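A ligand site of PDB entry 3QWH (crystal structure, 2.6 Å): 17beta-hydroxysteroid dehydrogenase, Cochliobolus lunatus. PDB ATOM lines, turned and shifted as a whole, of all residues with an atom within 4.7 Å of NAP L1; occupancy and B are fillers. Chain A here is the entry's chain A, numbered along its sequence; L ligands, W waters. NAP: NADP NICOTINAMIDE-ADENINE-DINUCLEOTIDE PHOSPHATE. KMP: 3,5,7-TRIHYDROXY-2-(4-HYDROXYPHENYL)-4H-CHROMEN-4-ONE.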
ATOM      1  N   GLY A  25      16.104  11.354 -26.003  1.00  0.00           N
ATOM      2  CA  GLY A  25      16.679  11.400 -24.661  1.00  0.00           C
ATOM      3  C   GLY A  25      17.299  12.756 -24.388  1.00  0.00           C
ATOM      4  O   GLY A  25      18.491  12.838 -24.070  1.00  0.00           O
ATOM      5  N   SER A  26      16.506  13.810 -24.539  1.00  0.00           N
ATOM      6  CA  SER A  26      16.978  15.169 -24.293  1.00  0.00           C
ATOM      7  C   SER A  26      16.482  15.720 -22.979  1.00  0.00           C
ATOM      8  O   SER A  26      16.648  16.906 -22.695  1.00  0.00           O
ATOM      9  CB  SER A  26      16.620  16.109 -25.439  1.00  0.00           C
ATOM     10  OG  SER A  26      15.317  15.843 -25.922  1.00  0.00           O
ATOM     11  N   GLY A  27      15.891  14.874 -22.154  1.00  0.00           N
ATOM     12  CA  GLY A  27      15.552  15.257 -20.792  1.00  0.00           C
ATOM     13  C   GLY A  27      16.770  15.614 -19.959  1.00  0.00           C
ATOM     14  O   GLY A  27      16.705  16.525 -19.116  1.00  0.00           O
ATOM     15  N   ARG A  28      17.882  14.914 -20.164  1.00  0.00           N
ATOM     16  CA  ARG A  28      19.066  15.181 -19.375  1.00  0.00           C
ATOM     17  C   ARG A  28      20.357  14.989 -20.180  1.00  0.00           C
ATOM     18  O   ARG A  28      20.308  14.575 -21.338  1.00  0.00           O
ATOM     19  CB  ARG A  28      19.053  14.350 -18.074  1.00  0.00           C
ATOM     20  CG  ARG A  28      19.247  12.860 -18.265  1.00  0.00           C
ATOM     21  CD  ARG A  28      19.060  12.063 -16.975  1.00  0.00           C
ATOM     22  NE  ARG A  28      18.831  10.653 -17.291  1.00  0.00           N
ATOM     23  CZ  ARG A  28      19.680   9.661 -17.061  1.00  0.00           C
ATOM     24  NH1 ARG A  28      20.844   9.872 -16.460  1.00  0.00           N
ATOM     25  NH2 ARG A  28      19.340   8.426 -17.411  1.00  0.00           N
ATOM     26  N   GLY A  29      21.499  15.340 -19.565  1.00  0.00           N
ATOM     27  CA  GLY A  29      22.819  15.131 -20.151  1.00  0.00           C
ATOM     28  C   GLY A  29      23.094  15.873 -21.453  1.00  0.00           C
ATOM     29  O   GLY A  29      22.673  17.010 -21.642  1.00  0.00           O
ATOM     30  N   ILE A  30      23.805  15.211 -22.358  1.00  0.00           N
ATOM     31  CA  ILE A  30      24.185  15.796 -23.632  1.00  0.00           C
ATOM     32  C   ILE A  30      22.970  16.181 -24.465  1.00  0.00           C
ATOM     33  O   ILE A  30      22.902  17.285 -25.027  1.00  0.00           O
ATOM     34  CB  ILE A  30      25.120  14.824 -24.414  1.00  0.00           C
ATOM     35  CG1 ILE A  30      26.494  14.761 -23.733  1.00  0.00           C
ATOM     36  CG2 ILE A  30      25.227  15.236 -25.877  1.00  0.00           C
ATOM     37  CD1 ILE A  30      27.447  13.639 -24.225  1.00  0.00           C
ATOM     38  N   GLY A  31      21.992  15.282 -24.532  1.00  0.00           N
ATOM     39  CA  GLY A  31      20.729  15.551 -25.213  1.00  0.00           C
ATOM     40  C   GLY A  31      20.083  16.846 -24.758  1.00  0.00           C
ATOM     41  O   GLY A  31      19.618  17.630 -25.590  1.00  0.00           O
ATOM     42  N   ASN A  48      12.400  14.418 -26.382  1.00  0.00           N
ATOM     43  CA  ASN A  48      12.079  13.039 -26.056  1.00  0.00           C
ATOM     44  C   ASN A  48      12.763  12.577 -24.764  1.00  0.00           C
ATOM     45  O   ASN A  48      13.905  12.964 -24.470  1.00  0.00           O
ATOM     46  CB  ASN A  48      12.465  12.116 -27.211  1.00  0.00           C
ATOM     47  CG  ASN A  48      12.469  10.643 -26.822  1.00  0.00           C
ATOM     48  OD1 ASN A  48      13.526  10.002 -26.800  1.00  0.00           O
ATOM     49  ND2 ASN A  48      11.285  10.117 -26.504  1.00  0.00           N
ATOM     50  N   TYR A  49      12.029  11.754 -24.013  1.00  0.00           N
ATOM     51  CA  TYR A  49      12.543  11.096 -22.807  1.00  0.00           C
ATOM     52  C   TYR A  49      11.914   9.713 -22.689  1.00  0.00           C
ATOM     53  O   TYR A  49      10.881   9.433 -23.317  1.00  0.00           O
ATOM     54  CB  TYR A  49      12.203  11.920 -21.559  1.00  0.00           C
ATOM     55  CG  TYR A  49      10.717  12.038 -21.276  1.00  0.00           C
ATOM     56  CD1 TYR A  49       9.938  13.008 -21.898  1.00  0.00           C
ATOM     57  CD2 TYR A  49      10.091  11.175 -20.373  1.00  0.00           C
ATOM     58  CE1 TYR A  49       8.578  13.122 -21.637  1.00  0.00           C
ATOM     59  CE2 TYR A  49       8.717  11.290 -20.095  1.00  0.00           C
ATOM     60  CZ  TYR A  49       7.974  12.263 -20.739  1.00  0.00           C
ATOM     61  OH  TYR A  49       6.627  12.378 -20.485  1.00  0.00           O
ATOM     62  N   ALA A  50      12.515   8.841 -21.878  1.00  0.00           N
ATOM     63  CA  ALA A  50      11.893   7.555 -21.575  1.00  0.00           C
ATOM     64  C   ALA A  50      11.341   7.526 -20.153  1.00  0.00           C
ATOM     65  O   ALA A  50      10.223   7.031 -19.929  1.00  0.00           O
ATOM     66  CB  ALA A  50      12.873   6.436 -21.779  1.00  0.00           C
ATOM     67  N   ASN A  51      12.119   8.057 -19.204  1.00  0.00           N
ATOM     68  CA  ASN A  51      11.773   7.999 -17.783  1.00  0.00           C
ATOM     69  C   ASN A  51      11.724   9.393 -17.145  1.00  0.00           C
ATOM     70  O   ASN A  51      10.746   9.740 -16.469  1.00  0.00           O
ATOM     71  CB  ASN A  51      12.718   7.055 -17.026  1.00  0.00           C
ATOM     72  CG  ASN A  51      12.923   5.678 -17.747  1.00  0.00           C
ATOM     73  OD1 ASN A  51      12.207   4.704 -17.473  1.00  0.00           O
ATOM     74  ND2 ASN A  51      13.892   5.616 -18.676  1.00  0.00           N
ATOM     75  N   SER A  52      12.754  10.202 -17.429  1.00  0.00           N
ATOM     76  CA  SER A  52      12.956  11.547 -16.859  1.00  0.00           C
ATOM     77  C   SER A  52      11.891  12.632 -17.149  1.00  0.00           C
ATOM     78  O   SER A  52      12.197  13.675 -17.725  1.00  0.00           O
ATOM     79  CB  SER A  52      14.329  12.069 -17.319  1.00  0.00           C
ATOM     80  OG  SER A  52      15.389  11.263 -16.837  1.00  0.00           O
ATOM     81  N   ALA A  75       8.713   8.442 -25.131  1.00  0.00           N
ATOM     82  CA  ALA A  75       8.833   7.291 -26.019  1.00  0.00           C
ATOM     83  C   ALA A  75      10.096   6.488 -25.708  1.00  0.00           C
ATOM     84  O   ALA A  75      11.180   7.053 -25.486  1.00  0.00           O
ATOM     85  CB  ALA A  75       8.816   7.719 -27.494  1.00  0.00           C
ATOM     86  N   ASP A  76       9.954   5.166 -25.660  1.00  0.00           N
ATOM     87  CA  ASP A  76      11.075   4.257 -25.414  1.00  0.00           C
ATOM     88  C   ASP A  76      11.759   3.919 -26.739  1.00  0.00           C
ATOM     89  O   ASP A  76      11.227   3.163 -27.555  1.00  0.00           O
ATOM     90  CB  ASP A  76      10.595   2.977 -24.711  1.00  0.00           C
ATOM     91  CG  ASP A  76      11.718   1.991 -24.403  1.00  0.00           C
ATOM     92  OD1 ASP A  76      12.908   2.284 -24.707  1.00  0.00           O
ATOM     93  OD2 ASP A  76      11.417   0.920 -23.852  1.00  0.00           O
ATOM     94  N   ILE A  77      12.938   4.496 -26.930  1.00  0.00           N
ATOM     95  CA  ILE A  77      13.652   4.384 -28.223  1.00  0.00           C
ATOM     96  C   ILE A  77      14.116   2.951 -28.576  1.00  0.00           C
ATOM     97  O   ILE A  77      14.584   2.708 -29.691  1.00  0.00           O
ATOM     98  CB  ILE A  77      14.787   5.453 -28.339  1.00  0.00           C
ATOM     99  CG1 ILE A  77      14.194   6.863 -28.411  1.00  0.00           C
ATOM    100  CG2 ILE A  77      15.642   5.207 -29.564  1.00  0.00           C
ATOM    101  CD1 ILE A  77      13.214   7.119 -29.611  1.00  0.00           C
ATOM    102  N   ARG A  78      13.963   2.002 -27.648  1.00  0.00           N
ATOM    103  CA  ARG A  78      14.252   0.592 -27.945  1.00  0.00           C
ATOM    104  C   ARG A  78      13.166  -0.013 -28.817  1.00  0.00           C
ATOM    105  O   ARG A  78      13.446  -0.913 -29.614  1.00  0.00           O
ATOM    106  CB  ARG A  78      14.400  -0.221 -26.661  1.00  0.00           C
ATOM    107  CG  ARG A  78      15.787  -0.154 -26.093  1.00  0.00           C
ATOM    108  CD  ARG A  78      15.892  -0.969 -24.811  1.00  0.00           C
ATOM    109  NE  ARG A  78      17.247  -0.886 -24.268  1.00  0.00           N
ATOM    110  CZ  ARG A  78      17.588  -0.158 -23.206  1.00  0.00           C
ATOM    111  NH1 ARG A  78      16.682   0.542 -22.546  1.00  0.00           N
ATOM    112  NH2 ARG A  78      18.860  -0.145 -22.803  1.00  0.00           N
ATOM    113  N   ASN A 103      20.405  10.828 -29.904  1.00  0.00           N
ATOM    114  CA  ASN A 103      21.341  11.006 -28.809  1.00  0.00           C
ATOM    115  C   ASN A 103      21.281   9.930 -27.714  1.00  0.00           C
ATOM    116  O   ASN A 103      22.307   9.606 -27.097  1.00  0.00           O
ATOM    117  CB  ASN A 103      21.113  12.388 -28.184  1.00  0.00           C
ATOM    118  CG  ASN A 103      21.514  12.437 -26.716  1.00  0.00           C
ATOM    119  OD1 ASN A 103      22.677  12.623 -26.390  1.00  0.00           O
ATOM    120  ND2 ASN A 103      20.542  12.236 -25.823  1.00  0.00           N
ATOM    121  N   SER A 104      20.082   9.399 -27.465  1.00  0.00           N
ATOM    122  CA  SER A 104      19.859   8.406 -26.410  1.00  0.00           C
ATOM    123  C   SER A 104      20.876   7.283 -26.493  1.00  0.00           C
ATOM    124  O   SER A 104      21.092   6.712 -27.561  1.00  0.00           O
ATOM    125  CB  SER A 104      18.463   7.803 -26.543  1.00  0.00           C
ATOM    126  OG  SER A 104      17.454   8.783 -26.370  1.00  0.00           O
ATOM    127  N   GLY A 105      21.495   6.957 -25.363  1.00  0.00           N
ATOM    128  CA  GLY A 105      22.440   5.864 -25.325  1.00  0.00           C
ATOM    129  C   GLY A 105      22.600   5.332 -23.930  1.00  0.00           C
ATOM    130  O   GLY A 105      22.154   5.978 -22.966  1.00  0.00           O
ATOM    131  N   VAL A 106      23.190   4.142 -23.814  1.00  0.00           N
ATOM    132  CA  VAL A 106      23.641   3.618 -22.508  1.00  0.00           C
ATOM    133  C   VAL A 106      25.055   3.038 -22.610  1.00  0.00           C
ATOM    134  O   VAL A 106      25.511   2.666 -23.710  1.00  0.00           O
ATOM    135  CB  VAL A 106      22.676   2.564 -21.898  1.00  0.00           C
ATOM    136  CG1 VAL A 106      21.414   3.212 -21.353  1.00  0.00           C
ATOM    137  CG2 VAL A 106      22.377   1.474 -22.904  1.00  0.00           C
ATOM    138  N   LEU A 126      19.336  -0.252 -27.937  1.00  0.00           N
ATOM    139  CA  LEU A 126      19.277   1.207 -27.856  1.00  0.00           C
ATOM    140  C   LEU A 126      20.333   1.903 -28.709  1.00  0.00           C
ATOM    141  O   LEU A 126      19.974   2.659 -29.618  1.00  0.00           O
ATOM    142  CB  LEU A 126      19.401   1.680 -26.418  1.00  0.00           C
ATOM    143  CG  LEU A 126      19.220   3.192 -26.271  1.00  0.00           C
ATOM    144  CD1 LEU A 126      17.823   3.653 -26.782  1.00  0.00           C
ATOM    145  CD2 LEU A 126      19.453   3.561 -24.815  1.00  0.00           C
ATOM    146  N   THR A 151      24.622   9.709 -32.616  1.00  0.00           N
ATOM    147  CA  THR A 151      25.626   9.848 -31.565  1.00  0.00           C
ATOM    148  C   THR A 151      26.503   8.605 -31.429  1.00  0.00           C
ATOM    149  O   THR A 151      26.002   7.494 -31.257  1.00  0.00           O
ATOM    150  CB  THR A 151      24.976  10.184 -30.240  1.00  0.00           C
ATOM    151  OG1 THR A 151      24.113  11.312 -30.442  1.00  0.00           O
ATOM    152  CG2 THR A 151      26.017  10.542 -29.218  1.00  0.00           C
ATOM    153  N   SER A 152      27.808   8.826 -31.517  1.00  0.00           N
ATOM    154  CA  SER A 152      28.811   7.775 -31.470  1.00  0.00           C
ATOM    155  C   SER A 152      29.703   8.022 -30.255  1.00  0.00           C
ATOM    156  O   SER A 152      29.299   8.732 -29.336  1.00  0.00           O
ATOM    157  CB  SER A 152      29.629   7.775 -32.776  1.00  0.00           C
ATOM    158  OG  SER A 152      30.548   6.690 -32.825  1.00  0.00           O
ATOM    159  N   SER A 153      30.909   7.469 -30.259  1.00  0.00           N
ATOM    160  CA  SER A 153      31.839   7.587 -29.141  1.00  0.00           C
ATOM    161  C   SER A 153      33.292   7.705 -29.641  1.00  0.00           C
ATOM    162  O   SER A 153      33.630   7.174 -30.689  1.00  0.00           O
ATOM    163  CB  SER A 153      31.708   6.360 -28.249  1.00  0.00           C
ATOM    164  OG  SER A 153      32.391   6.511 -27.015  1.00  0.00           O
ATOM    165  N   TYR A 167      30.316  -1.758 -25.875  1.00  0.00           N
ATOM    166  CA  TYR A 167      29.865  -0.386 -26.118  1.00  0.00           C
ATOM    167  C   TYR A 167      30.612   0.187 -27.312  1.00  0.00           C
ATOM    168  O   TYR A 167      30.039   0.918 -28.113  1.00  0.00           O
ATOM    169  CB  TYR A 167      30.091   0.477 -24.877  1.00  0.00           C
ATOM    170  CG  TYR A 167      29.786   1.946 -25.052  1.00  0.00           C
ATOM    171  CD1 TYR A 167      28.524   2.439 -24.815  1.00  0.00           C
ATOM    172  CD2 TYR A 167      30.784   2.856 -25.402  1.00  0.00           C
ATOM    173  CE1 TYR A 167      28.241   3.802 -24.969  1.00  0.00           C
ATOM    174  CE2 TYR A 167      30.525   4.214 -25.557  1.00  0.00           C
ATOM    175  CZ  TYR A 167      29.256   4.678 -25.337  1.00  0.00           C
ATOM    176  OH  TYR A 167      28.994   6.014 -25.489  1.00  0.00           O
ATOM    177  N   LYS A 171      28.840   1.523 -31.052  1.00  0.00           N
ATOM    178  CA  LYS A 171      29.031   2.804 -31.731  1.00  0.00           C
ATOM    179  C   LYS A 171      29.762   2.719 -33.089  1.00  0.00           C
ATOM    180  O   LYS A 171      29.489   3.510 -34.000  1.00  0.00           O
ATOM    181  CB  LYS A 171      29.696   3.809 -30.801  1.00  0.00           C
ATOM    182  CG  LYS A 171      28.909   4.056 -29.499  1.00  0.00           C
ATOM    183  CD  LYS A 171      27.436   4.341 -29.747  1.00  0.00           C
ATOM    184  CE  LYS A 171      26.769   4.851 -28.478  1.00  0.00           C
ATOM    185  NZ  LYS A 171      26.938   6.301 -28.288  1.00  0.00           N
ATOM    186  N   PRO A 197      31.643  12.029 -28.953  1.00  0.00           N
ATOM    187  CA  PRO A 197      32.311  12.731 -27.853  1.00  0.00           C
ATOM    188  C   PRO A 197      33.341  11.865 -27.162  1.00  0.00           C
ATOM    189  O   PRO A 197      33.243  10.651 -27.190  1.00  0.00           O
ATOM    190  CB  PRO A 197      31.159  13.028 -26.877  1.00  0.00           C
ATOM    191  CG  PRO A 197      29.907  12.884 -27.663  1.00  0.00           C
ATOM    192  CD  PRO A 197      30.218  11.802 -28.676  1.00  0.00           C
ATOM    193  N   GLY A 198      34.349  12.524 -26.587  1.00  0.00           N
ATOM    194  CA  GLY A 198      35.232  11.922 -25.596  1.00  0.00           C
ATOM    195  C   GLY A 198      34.524  12.025 -24.268  1.00  0.00           C
ATOM    196  O   GLY A 198      33.302  12.262 -24.217  1.00  0.00           O
ATOM    197  N   GLY A 199      35.270  11.854 -23.175  1.00  0.00           N
ATOM    198  CA  GLY A 199      34.711  11.984 -21.825  1.00  0.00           C
ATOM    199  C   GLY A 199      34.015  13.314 -21.621  1.00  0.00           C
ATOM    200  O   GLY A 199      34.662  14.344 -21.467  1.00  0.00           O
ATOM    201  N   THR A 200      32.686  13.273 -21.659  1.00  0.00           N
ATOM    202  CA  THR A 200      31.851  14.459 -21.477  1.00  0.00           C
ATOM    203  C   THR A 200      31.175  14.324 -20.104  1.00  0.00           C
ATOM    204  O   THR A 200      30.730  13.229 -19.734  1.00  0.00           O
ATOM    205  CB  THR A 200      30.798  14.589 -22.596  1.00  0.00           C
ATOM    206  OG1 THR A 200      31.424  14.469 -23.872  1.00  0.00           O
ATOM    207  CG2 THR A 200      30.085  15.904 -22.523  1.00  0.00           C
ATOM    208  N   THR A 202      28.530  14.159 -17.815  1.00  0.00           N
ATOM    209  CA  THR A 202      27.123  13.915 -17.540  1.00  0.00           C
ATOM    210  C   THR A 202      27.028  12.807 -16.481  1.00  0.00           C
ATOM    211  O   THR A 202      28.049  12.394 -15.931  1.00  0.00           O
ATOM    212  CB  THR A 202      26.365  13.482 -18.807  1.00  0.00           C
ATOM    213  OG1 THR A 202      26.823  12.185 -19.205  1.00  0.00           O
ATOM    214  CG2 THR A 202      26.585  14.447 -19.943  1.00  0.00           C
ATOM    215  N   ASP A 203      25.813  12.344 -16.177  1.00  0.00           N
ATOM    216  CA  ASP A 203      25.644  11.210 -15.266  1.00  0.00           C
ATOM    217  C   ASP A 203      26.457   9.993 -15.760  1.00  0.00           C
ATOM    218  O   ASP A 203      27.064   9.285 -14.954  1.00  0.00           O
ATOM    219  CB  ASP A 203      24.169  10.832 -15.143  1.00  0.00           C
ATOM    220  CG  ASP A 203      23.378  11.798 -14.270  1.00  0.00           C
ATOM    221  OD1 ASP A 203      23.880  12.194 -13.196  1.00  0.00           O
ATOM    222  OD2 ASP A 203      22.223  12.141 -14.653  1.00  0.00           O
ATOM    223  N   MET A 204      26.479   9.787 -17.074  1.00  0.00           N
ATOM    224  CA  MET A 204      27.225   8.678 -17.680  1.00  0.00           C
ATOM    225  C   MET A 204      28.717   8.729 -17.387  1.00  0.00           C
ATOM    226  O   MET A 204      29.351   7.706 -17.166  1.00  0.00           O
ATOM    227  CB  MET A 204      27.003   8.644 -19.190  1.00  0.00           C
ATOM    228  CG  MET A 204      27.696   7.469 -19.884  1.00  0.00           C
ATOM    229  SD  MET A 204      27.361   7.400 -21.637  1.00  0.00           S
ATOM    230  CE  MET A 204      25.622   6.960 -21.640  1.00  0.00           C
ATOM    231  N   PHE A 205      29.287   9.941 -17.409  1.00  0.00           N
ATOM    232  CA  PHE A 205      30.688  10.137 -17.093  1.00  0.00           C
ATOM    233  C   PHE A 205      30.943   9.537 -15.715  1.00  0.00           C
ATOM    234  O   PHE A 205      31.760   8.612 -15.587  1.00  0.00           O
ATOM    235  CB  PHE A 205      31.074  11.635 -17.145  1.00  0.00           C
ATOM    236  CG  PHE A 205      32.554  11.897 -16.894  1.00  0.00           C
ATOM    237  CD1 PHE A 205      33.469  11.887 -17.951  1.00  0.00           C
ATOM    238  CD2 PHE A 205      33.037  12.116 -15.612  1.00  0.00           C
ATOM    239  CE1 PHE A 205      34.821  12.110 -17.743  1.00  0.00           C
ATOM    240  CE2 PHE A 205      34.393  12.346 -15.384  1.00  0.00           C
ATOM    241  CZ  PHE A 205      35.289  12.336 -16.457  1.00  0.00           C
HETATM  242  PA  NAP L   1      23.300  10.159 -19.776  1.00  0.00           P
HETATM  243  O1A NAP L   1      23.133   8.866 -19.086  1.00  0.00           O
HETATM  244  O2A NAP L   1      23.640  11.374 -18.990  1.00  0.00           O
HETATM  245  O5B NAP L   1      21.950  10.414 -20.623  1.00  0.00           O
HETATM  246  C5B NAP L   1      21.278   9.322 -21.212  1.00  0.00           C
HETATM  247  C4B NAP L   1      20.079   9.790 -22.006  1.00  0.00           C
HETATM  248  O4B NAP L   1      19.704   8.569 -22.683  1.00  0.00           O
HETATM  249  C3B NAP L   1      18.887  10.199 -21.123  1.00  0.00           C
HETATM  250  O3B NAP L   1      18.232  11.341 -21.659  1.00  0.00           O
HETATM  251  C2B NAP L   1      17.951   8.989 -21.210  1.00  0.00           C
HETATM  252  O2B NAP L   1      16.577   9.368 -21.059  1.00  0.00           O
HETATM  253  C1B NAP L   1      18.255   8.477 -22.640  1.00  0.00           C
HETATM  254  N9A NAP L   1      17.712   7.094 -22.699  1.00  0.00           N
HETATM  255  C8A NAP L   1      18.149   6.029 -22.004  1.00  0.00           C
HETATM  256  N7A NAP L   1      17.375   4.978 -22.280  1.00  0.00           N
HETATM  257  C5A NAP L   1      16.452   5.375 -23.161  1.00  0.00           C
HETATM  258  C6A NAP L   1      15.392   4.738 -23.823  1.00  0.00           C
HETATM  259  N6A NAP L   1      15.143   3.450 -23.613  1.00  0.00           N
HETATM  260  N1A NAP L   1      14.629   5.454 -24.671  1.00  0.00           N
HETATM  261  C2A NAP L   1      14.868   6.738 -24.883  1.00  0.00           C
HETATM  262  N3A NAP L   1      15.853   7.379 -24.280  1.00  0.00           N
HETATM  263  C4A NAP L   1      16.658   6.722 -23.420  1.00  0.00           C
HETATM  264  O3  NAP L   1      24.389   9.971 -20.928  1.00  0.00           O
HETATM  265  PN  NAP L   1      24.997  11.194 -21.846  1.00  0.00           P
HETATM  266  O1N NAP L   1      24.172  12.434 -21.738  1.00  0.00           O
HETATM  267  O2N NAP L   1      26.439  11.264 -21.552  1.00  0.00           O
HETATM  268  O5D NAP L   1      24.785  10.480 -23.278  1.00  0.00           O
HETATM  269  C5D NAP L   1      24.514  11.089 -24.513  1.00  0.00           C
HETATM  270  C4D NAP L   1      25.064  10.192 -25.664  1.00  0.00           C
HETATM  271  O4D NAP L   1      26.499  10.459 -25.860  1.00  0.00           O
HETATM  272  C3D NAP L   1      24.938   8.654 -25.495  1.00  0.00           C
HETATM  273  O3D NAP L   1      24.521   8.075 -26.736  1.00  0.00           O
HETATM  274  C2D NAP L   1      26.355   8.209 -25.186  1.00  0.00           C
HETATM  275  O2D NAP L   1      26.585   6.904 -25.710  1.00  0.00           O
HETATM  276  C1D NAP L   1      27.187   9.203 -25.966  1.00  0.00           C
HETATM  277  N1N NAP L   1      28.522   9.406 -25.339  1.00  0.00           N
HETATM  278  C2N NAP L   1      28.674  10.005 -24.071  1.00  0.00           C
HETATM  279  C3N NAP L   1      29.960  10.171 -23.549  1.00  0.00           C
HETATM  280  C7N NAP L   1      30.227  10.811 -22.188  1.00  0.00           C
HETATM  281  O7N NAP L   1      31.468  10.832 -21.668  1.00  0.00           O
HETATM  282  N7N NAP L   1      29.215  11.406 -21.560  1.00  0.00           N
HETATM  283  C4N NAP L   1      31.065   9.753 -24.285  1.00  0.00           C
HETATM  284  C5N NAP L   1      30.914   9.170 -25.535  1.00  0.00           C
HETATM  285  C6N NAP L   1      29.646   8.994 -26.071  1.00  0.00           C
HETATM  286  P2B NAP L   1      15.727   8.888 -19.759  1.00  0.00           P
HETATM  287  O1X NAP L   1      14.439   9.605 -19.616  1.00  0.00           O
HETATM  288  O2X NAP L   1      16.681   9.043 -18.480  1.00  0.00           O
HETATM  289  O3X NAP L   1      15.515   7.303 -19.888  1.00  0.00           O
HETATM  290  C1  KMP L   2      33.669   8.325 -21.815  1.00  0.00           C
HETATM  291  C2  KMP L   2      34.092   8.481 -20.506  1.00  0.00           C
HETATM  292  C3  KMP L   2      35.441   8.782 -20.221  1.00  0.00           C
HETATM  293  C4  KMP L   2      36.361   8.913 -21.287  1.00  0.00           C
HETATM  294  C5  KMP L   2      35.908   8.756 -22.606  1.00  0.00           C
HETATM  295  C6  KMP L   2      34.562   8.462 -22.870  1.00  0.00           C
HETATM  296  C9  KMP L   2      35.899   8.928 -18.909  1.00  0.00           C
HETATM  297  C10 KMP L   2      37.256   9.182 -18.675  1.00  0.00           C
HETATM  298  C11 KMP L   2      38.152   9.317 -19.739  1.00  0.00           C
HETATM  299  C14 KMP L   2      39.525   9.530 -19.512  1.00  0.00           C
HETATM  300  C15 KMP L   2      40.061   9.570 -18.224  1.00  0.00           C
HETATM  301  C16 KMP L   2      41.421   9.765 -18.008  1.00  0.00           C
HETATM  302  C17 KMP L   2      42.291   9.897 -19.091  1.00  0.00           C
HETATM  303  C18 KMP L   2      41.785   9.842 -20.386  1.00  0.00           C
HETATM  304  C19 KMP L   2      40.409   9.654 -20.599  1.00  0.00           C
HETATM  305  O12 KMP L   2      37.695   9.195 -21.046  1.00  0.00           O
HETATM  306  O13 KMP L   2      35.113   8.808 -17.963  1.00  0.00           O
HETATM  307  O24 KMP L   2      43.624  10.082 -18.881  1.00  0.00           O
HETATM  308  O27 KMP L   2      37.710   9.296 -17.388  1.00  0.00           O
HETATM  309  O29 KMP L   2      34.100   8.297 -24.136  1.00  0.00           O
HETATM  310  O30 KMP L   2      33.174   8.329 -19.509  1.00  0.00           O
HETATM  311  O   HOH W   1      22.832   7.675 -16.738  1.00  0.00           O
HETATM  312  O   HOH W   2      23.346  13.448 -17.061  1.00  0.00           O
HETATM  313  O   HOH W   3      15.536  12.038 -20.991  1.00  0.00           O
HETATM  314  O   HOH W   4      13.803   0.817 -22.108  1.00  0.00           O
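The backbone NH (N) of Ser 52 sits at hydrogen-bond distance from an oxygen (O1X) of NAP L1.
ND2 of Asn 51 is in hydrogen-bond range of O3X of NAP L1 (2.6 Å).
A nitrogen (N3A) of NAP L1 sits at hydrogen-bond distance from the side-chain hydroxyl (OG) of Ser 104.
The backbone NH (N) of Ile 30 lies within hydrogen-bond range of an oxygen (O1N) of NAP L1 (2.9 Å).
An oxygen (O2D) of NAP L1 lies within hydrogen-bond range of the side-chain hydroxyl (OH) of Tyr 167 (2.6 Å).
An oxygen (O2D) of NAP L1 sits at hydrogen-bond distance from the side-chain amino group of Lys 171, 2.7 Å away.
NH2 of Arg 28 lies within salt-bridge range of O2X of NAP L1 (2.9 Å).
O of Thr 200 sits at hydrogen-bond distance from N7N of NAP L1 (3.0 Å).
A nitrogen (N6A) of NAP L1 lies within hydrogen-bond range of the side-chain carboxylate (OD1) of Asp 76, 2.7 Å away.
The backbone carbonyl oxygen of Gly 25 lies within hydrogen-bond range of an oxygen (O3B) of NAP L1 (2.8 Å).
An oxygen (O3D) of NAP L1 sits at hydrogen-bond distance from the backbone carbonyl oxygen (O) of Asn 103.
OG1 of Thr 202 sits at hydrogen-bond distance from O2N of NAP L1 (2.6 Å).
N of Asn 51 is in hydrogen-bond range of O1X of NAP L1 (2.8 Å).
The backbone NH of Thr 200 is in hydrogen-bond range of an oxygen (O7N) of NAP L1, 2.7 Å away.
The side-chain hydroxyl (OG) of Ser 52 sits at hydrogen-bond distance from an oxygen (O2X) of NAP L1 (3.0 Å).
N of Ile 77 lies within hydrogen-bond range of N1A of NAP L1.
An oxygen (O1X) of NAP L1 lies within hydrogen-bond range of the backbone NH of Ala 50, 3.1 Å away.
Water W1 lies within hydrogen-bond range of an oxygen (O1A) of NAP L1 (2.6 Å) and the guanidinium group of Arg 28 (3.0 Å).
Water W2 lies within hydrogen-bond range of N of Asp 203 (2.8 Å) and O2A of NAP L1 (2.8 Å).
Water W3 bridges an oxygen (O3B) of NAP L1 and the backbone NH of Gly 27.
Water W4 lies within hydrogen-bond range of NH1 of Arg 78 (2.9 Å), OD2 of Asp 76 (3.0 Å) and N6A of NAP L1 (3.3 Å).
NZ of Lys 171 is in hydrogen-bond range of OH of Tyr 167 (3.5 Å).
The backbone NH of Met 204 sits close to the side-chain hydroxyl of Thr 202, at 3.2 Å.
O of Ala 75 is in hydrogen-bond range of ND2 of Asn 48.
NZ of Lys 171 lies within hydrogen-bond range of O of Thr 151 (3.3 Å).
N of Ala 75 is in hydrogen-bond range of O of Tyr 49, at 3.0 Å.
OD1 of Asn 103 is in hydrogen-bond range of N of Gly 31 (3.3 Å).
The backbone carbonyl oxygen (O) of Gly 198 is in hydrogen-bond range of the side-chain hydroxyl (OG1) of Thr 200 (2.9 Å).
N of Gly 25 sits at hydrogen-bond distance from OG of Ser 104, 2.9 Å away.
NH1 of Arg 78 lies close to N6A of NAP L1.
O of Gly 198 lies close to O7N of NAP L1, 3.5 Å away.
CA of Gly 29 touches O1N of NAP L1 (3.4 Å).
CB of Tyr 49 touches O1X of NAP L1 (3.8 Å).
Ala 75 touches NAP L1 (O to C2A, 3.8 Å).
Gly 105 touches NAP L1.
CD2 of Leu 126 touches N7A of NAP L1, 3.6 Å away.
CG2 of Thr 151 touches O4D of NAP L1, 3.4 Å away.
O of Ser 152 touches C6N of NAP L1 (3.3 Å).
OG of Ser 153 touches C5N of NAP L1, at 3.4 Å.
O of Pro 197 touches C5N of NAP L1, at 3.2 Å.
CA of Gly 199 touches O7N of NAP L1 (3.4 Å).
N of Asp 203 touches O2A of NAP L1 (3.7 Å).
Met 204 touches NAP L1 (CE to O3, 3.3 Å).
Within 4 Å of NAP L1: Gly 25, Arg 28, Gly 29, Ile 30, Tyr 49, Ala 50, Asn 51, Ser 52, Ala 75, Asp 76, Ile 77, Arg 78, Asn 103, Ser 104, Gly 105, Leu 126, Thr 151, Ser 152, Ser 153, Tyr 167, Lys 171, Pro 197, Gly 198, Gly 199, Thr 200, Thr 202, Asp 203 and Met 204.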
